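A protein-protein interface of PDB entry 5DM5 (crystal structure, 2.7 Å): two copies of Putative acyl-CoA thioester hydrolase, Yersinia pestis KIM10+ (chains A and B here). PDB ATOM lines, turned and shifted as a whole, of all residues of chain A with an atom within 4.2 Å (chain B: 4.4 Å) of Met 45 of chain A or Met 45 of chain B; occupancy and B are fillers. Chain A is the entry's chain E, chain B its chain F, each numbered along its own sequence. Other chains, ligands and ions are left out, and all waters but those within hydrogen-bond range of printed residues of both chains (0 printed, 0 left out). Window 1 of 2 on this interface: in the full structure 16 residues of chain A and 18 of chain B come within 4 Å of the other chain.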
ATOM      1  N   GLY A  41     -24.551  10.625 -19.636  1.00  0.00           N
ATOM      2  CA  GLY A  41     -25.526  11.053 -18.641  1.00  0.00           C
ATOM      3  C   GLY A  41     -25.005  11.050 -17.225  1.00  0.00           C
ATOM      4  O   GLY A  41     -25.431  11.829 -16.381  1.00  0.00           O
ATOM      5  N   GLY A  42     -24.058  10.174 -16.966  1.00  0.00           N
ATOM      6  CA  GLY A  42     -22.997  10.474 -16.037  1.00  0.00           C
ATOM      7  C   GLY A  42     -22.640  11.938 -16.009  1.00  0.00           C
ATOM      8  O   GLY A  42     -22.704  12.560 -14.959  1.00  0.00           O
ATOM      9  N   TRP A  43     -22.284  12.504 -17.161  1.00  0.00           N
ATOM     10  CA  TRP A  43     -21.845  13.896 -17.186  1.00  0.00           C
ATOM     11  C   TRP A  43     -22.924  14.880 -16.809  1.00  0.00           C
ATOM     12  O   TRP A  43     -22.665  15.844 -16.107  1.00  0.00           O
ATOM     13  CB  TRP A  43     -21.312  14.284 -18.556  1.00  0.00           C
ATOM     14  CG  TRP A  43     -20.847  15.688 -18.578  1.00  0.00           C
ATOM     15  CD1 TRP A  43     -19.667  16.146 -18.079  1.00  0.00           C
ATOM     16  CD2 TRP A  43     -21.510  16.830 -19.152  1.00  0.00           C
ATOM     17  NE1 TRP A  43     -19.555  17.503 -18.282  1.00  0.00           N
ATOM     18  CE2 TRP A  43     -20.666  17.948 -18.947  1.00  0.00           C
ATOM     19  CE3 TRP A  43     -22.723  17.021 -19.814  1.00  0.00           C
ATOM     20  CZ2 TRP A  43     -21.001  19.239 -19.380  1.00  0.00           C
ATOM     21  CZ3 TRP A  43     -23.053  18.313 -20.245  1.00  0.00           C
ATOM     22  CH2 TRP A  43     -22.197  19.397 -20.021  1.00  0.00           C
ATOM     23  N   LEU A  44     -24.139  14.612 -17.253  1.00  0.00           N
ATOM     24  CA  LEU A  44     -25.261  15.465 -16.937  1.00  0.00           C
ATOM     25  C   LEU A  44     -25.458  15.513 -15.448  1.00  0.00           C
ATOM     26  O   LEU A  44     -25.534  16.576 -14.855  1.00  0.00           O
ATOM     27  CB  LEU A  44     -26.527  14.950 -17.612  1.00  0.00           C
ATOM     28  CG  LEU A  44     -26.776  15.224 -19.105  1.00  0.00           C
ATOM     29  CD1 LEU A  44     -26.682  16.699 -19.424  1.00  0.00           C
ATOM     30  CD2 LEU A  44     -25.832  14.437 -19.998  1.00  0.00           C
ATOM     31  N   MET A  45     -25.489  14.341 -14.845  1.00  0.00           N
ATOM     32  CA  MET A  45     -25.630  14.213 -13.404  1.00  0.00           C
ATOM     33  C   MET A  45     -24.474  14.861 -12.652  1.00  0.00           C
ATOM     34  O   MET A  45     -24.632  15.333 -11.523  1.00  0.00           O
ATOM     35  CB  MET A  45     -25.721  12.746 -13.044  1.00  0.00           C
ATOM     36  CG  MET A  45     -26.785  11.991 -13.795  1.00  0.00           C
ATOM     37  SD  MET A  45     -26.933  10.281 -13.276  1.00  0.00           S
ATOM     38  CE  MET A  45     -25.291   9.719 -13.605  1.00  0.00           C
ATOM     39  N   SER A  46     -23.298  14.808 -13.272  1.00  0.00           N
ATOM     40  CA  SER A  46     -22.092  15.442 -12.755  1.00  0.00           C
ATOM     41  C   SER A  46     -22.259  16.947 -12.698  1.00  0.00           C
ATOM     42  O   SER A  46     -21.820  17.597 -11.749  1.00  0.00           O
ATOM     43  CB  SER A  46     -20.878  15.106 -13.615  1.00  0.00           C
ATOM     44  OG  SER A  46     -20.688  13.713 -13.692  1.00  0.00           O
ATOM     45  N   GLN A  47     -22.835  17.508 -13.754  1.00  0.00           N
ATOM     46  CA  GLN A  47     -23.082  18.934 -13.801  1.00  0.00           C
ATOM     47  C   GLN A  47     -24.149  19.315 -12.777  1.00  0.00           C
ATOM     48  O   GLN A  47     -24.050  20.339 -12.106  1.00  0.00           O
ATOM     49  CB  GLN A  47     -23.499  19.357 -15.196  1.00  0.00           C
ATOM     50  CG  GLN A  47     -22.504  18.898 -16.224  1.00  0.00           C
ATOM     51  CD  GLN A  47     -21.105  19.391 -15.949  1.00  0.00           C
ATOM     52  OE1 GLN A  47     -20.179  18.587 -15.780  1.00  0.00           O
ATOM     53  NE2 GLN A  47     -20.936  20.707 -15.889  1.00  0.00           N
ATOM     54  N   MET A  48     -25.174  18.482 -12.654  1.00  0.00           N
ATOM     55  CA  MET A  48     -26.245  18.756 -11.703  1.00  0.00           C
ATOM     56  C   MET A  48     -25.722  18.735 -10.263  1.00  0.00           C
ATOM     57  O   MET A  48     -26.113  19.568  -9.460  1.00  0.00           O
ATOM     58  CB  MET A  48     -27.399  17.771 -11.882  1.00  0.00           C
ATOM     59  CG  MET A  48     -27.941  17.722 -13.309  1.00  0.00           C
ATOM     60  SD  MET A  48     -29.361  16.650 -13.587  1.00  0.00           S
ATOM     61  CE  MET A  48     -30.638  17.507 -12.701  1.00  0.00           C
ATOM     62  N   ASP A  49     -24.804  17.823  -9.955  1.00  0.00           N
ATOM     63  CA  ASP A  49     -24.179  17.790  -8.630  1.00  0.00           C
ATOM     64  C   ASP A  49     -23.616  19.153  -8.239  1.00  0.00           C
ATOM     65  O   ASP A  49     -23.865  19.658  -7.143  1.00  0.00           O
ATOM     66  CB  ASP A  49     -23.030  16.773  -8.652  1.00  0.00           C
ATOM     67  CG  ASP A  49     -22.306  16.638  -7.316  1.00  0.00           C
ATOM     68  OD1 ASP A  49     -21.324  15.880  -7.275  1.00  0.00           O
ATOM     69  OD2 ASP A  49     -22.602  17.364  -6.351  1.00  0.00           O
ATOM     70  N   MET A  72     -34.468  11.421 -10.328  1.00  0.00           N
ATOM     71  CA  MET A  72     -33.745  11.969 -11.461  1.00  0.00           C
ATOM     72  C   MET A  72     -34.316  11.458 -12.764  1.00  0.00           C
ATOM     73  O   MET A  72     -34.498  10.270 -12.966  1.00  0.00           O
ATOM     74  CB  MET A  72     -32.258  11.642 -11.407  1.00  0.00           C
ATOM     75  CG  MET A  72     -31.523  12.156 -12.630  1.00  0.00           C
ATOM     76  SD  MET A  72     -29.760  12.318 -12.414  1.00  0.00           S
ATOM     77  CE  MET A  72     -29.641  13.514 -11.095  1.00  0.00           C
ATOM     78  N   PHE A  74     -34.155  11.690 -17.040  1.00  0.00           N
ATOM     79  CA  PHE A  74     -33.586  12.099 -18.326  1.00  0.00           C
ATOM     80  C   PHE A  74     -34.641  12.205 -19.407  1.00  0.00           C
ATOM     81  O   PHE A  74     -35.062  11.200 -19.942  1.00  0.00           O
ATOM     82  CB  PHE A  74     -32.488  11.148 -18.792  1.00  0.00           C
ATOM     83  CG  PHE A  74     -31.273  11.157 -17.921  1.00  0.00           C
ATOM     84  CD1 PHE A  74     -30.268  12.090 -18.133  1.00  0.00           C
ATOM     85  CD2 PHE A  74     -31.132  10.241 -16.895  1.00  0.00           C
ATOM     86  CE1 PHE A  74     -29.154  12.099 -17.339  1.00  0.00           C
ATOM     87  CE2 PHE A  74     -30.017  10.241 -16.101  1.00  0.00           C
ATOM     88  CZ  PHE A  74     -29.027  11.167 -16.319  1.00  0.00           C
ATOM     89  N   GLY B  41     -18.413  14.144  -6.352  1.00  0.00           N
ATOM     90  CA  GLY B  41     -19.554  13.254  -6.167  1.00  0.00           C
ATOM     91  C   GLY B  41     -20.575  13.094  -7.275  1.00  0.00           C
ATOM     92  O   GLY B  41     -21.595  12.440  -7.085  1.00  0.00           O
ATOM     93  N   GLY B  42     -20.314  13.687  -8.429  1.00  0.00           N
ATOM     94  CA  GLY B  42     -21.122  13.421  -9.594  1.00  0.00           C
ATOM     95  C   GLY B  42     -20.400  12.360 -10.388  1.00  0.00           C
ATOM     96  O   GLY B  42     -20.978  11.660 -11.218  1.00  0.00           O
ATOM     97  N   TRP B  43     -19.103  12.256 -10.136  1.00  0.00           N
ATOM     98  CA  TRP B  43     -18.267  11.311 -10.859  1.00  0.00           C
ATOM     99  C   TRP B  43     -18.658   9.879 -10.506  1.00  0.00           C
ATOM    100  O   TRP B  43     -18.583   8.979 -11.346  1.00  0.00           O
ATOM    101  CB  TRP B  43     -16.791  11.556 -10.576  1.00  0.00           C
ATOM    102  CG  TRP B  43     -15.944  10.648 -11.361  1.00  0.00           C
ATOM    103  CD1 TRP B  43     -15.599  10.789 -12.674  1.00  0.00           C
ATOM    104  CD2 TRP B  43     -15.349   9.429 -10.916  1.00  0.00           C
ATOM    105  NE1 TRP B  43     -14.811   9.736 -13.071  1.00  0.00           N
ATOM    106  CE2 TRP B  43     -14.642   8.885 -12.007  1.00  0.00           C
ATOM    107  CE3 TRP B  43     -15.338   8.745  -9.699  1.00  0.00           C
ATOM    108  CZ2 TRP B  43     -13.926   7.692 -11.914  1.00  0.00           C
ATOM    109  CZ3 TRP B  43     -14.631   7.563  -9.609  1.00  0.00           C
ATOM    110  CH2 TRP B  43     -13.933   7.049 -10.708  1.00  0.00           C
ATOM    111  N   LEU B  44     -19.049   9.680  -9.249  1.00  0.00           N
ATOM    112  CA  LEU B  44     -19.560   8.397  -8.790  1.00  0.00           C
ATOM    113  C   LEU B  44     -20.750   8.074  -9.640  1.00  0.00           C
ATOM    114  O   LEU B  44     -20.873   6.969 -10.117  1.00  0.00           O
ATOM    115  CB  LEU B  44     -20.010   8.434  -7.338  1.00  0.00           C
ATOM    116  CG  LEU B  44     -18.994   8.350  -6.222  1.00  0.00           C
ATOM    117  CD1 LEU B  44     -18.142   7.128  -6.438  1.00  0.00           C
ATOM    118  CD2 LEU B  44     -18.176   9.615  -6.201  1.00  0.00           C
ATOM    119  N   MET B  45     -21.617   9.070  -9.826  1.00  0.00           N
ATOM    120  CA  MET B  45     -22.810   8.924 -10.639  1.00  0.00           C
ATOM    121  C   MET B  45     -22.410   8.536 -12.051  1.00  0.00           C
ATOM    122  O   MET B  45     -23.111   7.769 -12.696  1.00  0.00           O
ATOM    123  CB  MET B  45     -23.617  10.216 -10.691  1.00  0.00           C
ATOM    124  CG  MET B  45     -23.961  10.843  -9.375  1.00  0.00           C
ATOM    125  SD  MET B  45     -24.996  12.298  -9.641  1.00  0.00           S
ATOM    126  CE  MET B  45     -26.571  11.548 -10.108  1.00  0.00           C
ATOM    127  N   SER B  46     -21.277   9.063 -12.515  1.00  0.00           N
ATOM    128  CA  SER B  46     -20.729   8.744 -13.833  1.00  0.00           C
ATOM    129  C   SER B  46     -20.379   7.266 -13.927  1.00  0.00           C
ATOM    130  O   SER B  46     -20.648   6.591 -14.934  1.00  0.00           O
ATOM    131  CB  SER B  46     -19.488   9.588 -14.097  1.00  0.00           C
ATOM    132  OG  SER B  46     -19.785  10.964 -13.955  1.00  0.00           O
ATOM    133  N   GLN B  47     -19.753   6.782 -12.864  1.00  0.00           N
ATOM    134  CA  GLN B  47     -19.379   5.383 -12.735  1.00  0.00           C
ATOM    135  C   GLN B  47     -20.572   4.449 -12.637  1.00  0.00           C
ATOM    136  O   GLN B  47     -20.612   3.401 -13.273  1.00  0.00           O
ATOM    137  CB  GLN B  47     -18.482   5.206 -11.510  1.00  0.00           C
ATOM    138  CG  GLN B  47     -17.142   5.910 -11.624  1.00  0.00           C
ATOM    139  CD  GLN B  47     -16.286   5.314 -12.731  1.00  0.00           C
ATOM    140  OE1 GLN B  47     -15.685   4.249 -12.558  1.00  0.00           O
ATOM    141  NE2 GLN B  47     -16.245   5.982 -13.880  1.00  0.00           N
ATOM    142  N   MET B  48     -21.551   4.855 -11.851  1.00  0.00           N
ATOM    143  CA  MET B  48     -22.747   4.077 -11.634  1.00  0.00           C
ATOM    144  C   MET B  48     -23.478   3.975 -12.929  1.00  0.00           C
ATOM    145  O   MET B  48     -23.967   2.923 -13.301  1.00  0.00           O
ATOM    146  CB  MET B  48     -23.596   4.743 -10.571  1.00  0.00           C
ATOM    147  CG  MET B  48     -22.808   4.959  -9.294  1.00  0.00           C
ATOM    148  SD  MET B  48     -23.685   5.756  -7.959  1.00  0.00           S
ATOM    149  CE  MET B  48     -24.879   4.443  -7.720  1.00  0.00           C
ATOM    150  N   ASP B  49     -23.508   5.078 -13.647  1.00  0.00           N
ATOM    151  CA  ASP B  49     -24.150   5.074 -14.931  1.00  0.00           C
ATOM    152  C   ASP B  49     -23.457   4.106 -15.865  1.00  0.00           C
ATOM    153  O   ASP B  49     -24.118   3.301 -16.519  1.00  0.00           O
ATOM    154  CB  ASP B  49     -24.137   6.453 -15.576  1.00  0.00           C
ATOM    155  CG  ASP B  49     -24.961   6.492 -16.844  1.00  0.00           C
ATOM    156  OD1 ASP B  49     -24.470   6.927 -17.918  1.00  0.00           O
ATOM    157  OD2 ASP B  49     -26.138   6.090 -16.739  1.00  0.00           O
ATOM    158  N   VAL B  69     -32.809   7.920 -12.595  1.00  0.00           N
ATOM    159  CA  VAL B  69     -32.018   7.621 -11.400  1.00  0.00           C
ATOM    160  C   VAL B  69     -32.898   7.914 -10.185  1.00  0.00           C
ATOM    161  O   VAL B  69     -33.266   9.056  -9.956  1.00  0.00           O
ATOM    162  CB  VAL B  69     -30.727   8.501 -11.295  1.00  0.00           C
ATOM    163  CG1 VAL B  69     -29.969   8.205  -9.998  1.00  0.00           C
ATOM    164  CG2 VAL B  69     -29.826   8.316 -12.494  1.00  0.00           C
ATOM    165  N   MET B  72     -30.834   7.523  -4.973  1.00  0.00           N
ATOM    166  CA  MET B  72     -29.402   7.354  -4.768  1.00  0.00           C
ATOM    167  C   MET B  72     -28.976   7.883  -3.410  1.00  0.00           C
ATOM    168  O   MET B  72     -29.227   9.035  -3.097  1.00  0.00           O
ATOM    169  CB  MET B  72     -28.592   8.065  -5.841  1.00  0.00           C
ATOM    170  CG  MET B  72     -27.088   7.896  -5.611  1.00  0.00           C
ATOM    171  SD  MET B  72     -26.046   8.241  -7.029  1.00  0.00           S
ATOM    172  CE  MET B  72     -26.612   9.890  -7.295  1.00  0.00           C
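Printed residues of chain B within 4 Å of Met 45 of chain A: Met 45, Asp 49 and Val 69. Of chain A, only Met 45 and Met 72 come within 4 Å of Met 45 of chain B. Of the printed residues of chain A, Gly 42 of chain B touches Ser 46 and Asp 49. Printed residues of chain A within 4 Å of Ser 46 of chain B: Gly 42 (3.5 Å) and Ser 46 (2.9 Å). Printed residues of chain B within 4 Å of Met 72 of chain A: Met 45 and Val 69. Printed residues of chain A within 4 Å of Gly 41 of chain B: Asp 49. Of the printed residues of chain A, Asp 49 of chain B touches Gly 42 (3.4 Å) and Met 45 (3.99 Å). Met 72 of chain B touches none of the printed residues of chain A. Gln 47 of chain A touches none of the printed residues of chain B. The nearest printed residue of chain A that does not touch Met 45 of chain B is Gly 42 of chain A (4.3 Å).
The backbone NH (N) of Met 72 of chain A sits at hydrogen-bond distance from the backbone carbonyl oxygen (O) of Val 69 of chain B (2.7 Å). The side-chain carboxylate (OD1) of Asp 49 of chain B is in hydrogen-bond range of the backbone NH (N) of Gly 42 of chain A. O of Gly 41 of chain B sits close to OD1 of Asp 49 of chain A (3.5 Å). N of Gly 42 of chain B sits at hydrogen-bond distance from OD1 of Asp 49 of chain A, 2.7 Å away. The backbone carbonyl oxygen of Gly 42 of chain A is in hydrogen-bond range of the side-chain hydroxyl of Ser 46 of chain B (3.5 Å). The side-chain hydroxyl of Ser 46 of chain A lies within hydrogen-bond range of the backbone carbonyl oxygen of Gly 42 of chain B. SD of Met 45 of chain B sits close to O of Met 45 of chain A, 3.6 Å away. The side-chain hydroxyl (OG) of Ser 46 of chain B lies within hydrogen-bond range of the side-chain hydroxyl (OG) of Ser 46 of chain A.
OG of Ser 46 of chain B is in hydrogen-bond range of O of Gly 42 of chain B, 3.1 Å away. O of Gly 42 of chain A lies within hydrogen-bond range of OG of Ser 46 of chain A, at 2.6 Å. O of Trp 43 of chain B lies close to OG of Ser 46 of chain B, 3.5 Å away.
Gly 42 of chain A touches Asp 49 of chain B, and with the chains exchanged Asp 49 of chain A touches Gly 42 of chain B. Met 45 of chain B touches its own counterpart, Met 45 of chain A. Met 45 of chain A touches Asp 49 of chain B, but with the chains exchanged Asp 49 of chain A does not touch Met 45 of chain B (5.0 Å). Asp 49 of chain A touches Gly 41 of chain B, but with the chains exchanged Gly 41 of chain A does not touch Asp 49 of chain B (4.1 Å).
Among the printed residues, merely in contact across the chains: Met 45 of chain A with Val 69 of chain B (3.6 Å), Met 72 of chain A with Met 45 of chain B (3.8 Å) and Met 45 of chain A with Asp 49 of chain B (3.99 Å).
Of the 11 printed residues of chain B, 6 touch a printed residue of chain A. Of the 11 printed residues of chain A, 5 touch a printed residue of chain B. Printed residues of chain A that touch a printed residue of chain B: Gly 42, Met 45, Ser 46, Asp 49 and Met 72. Among the printed residues, 11 pairs touch across the chains.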
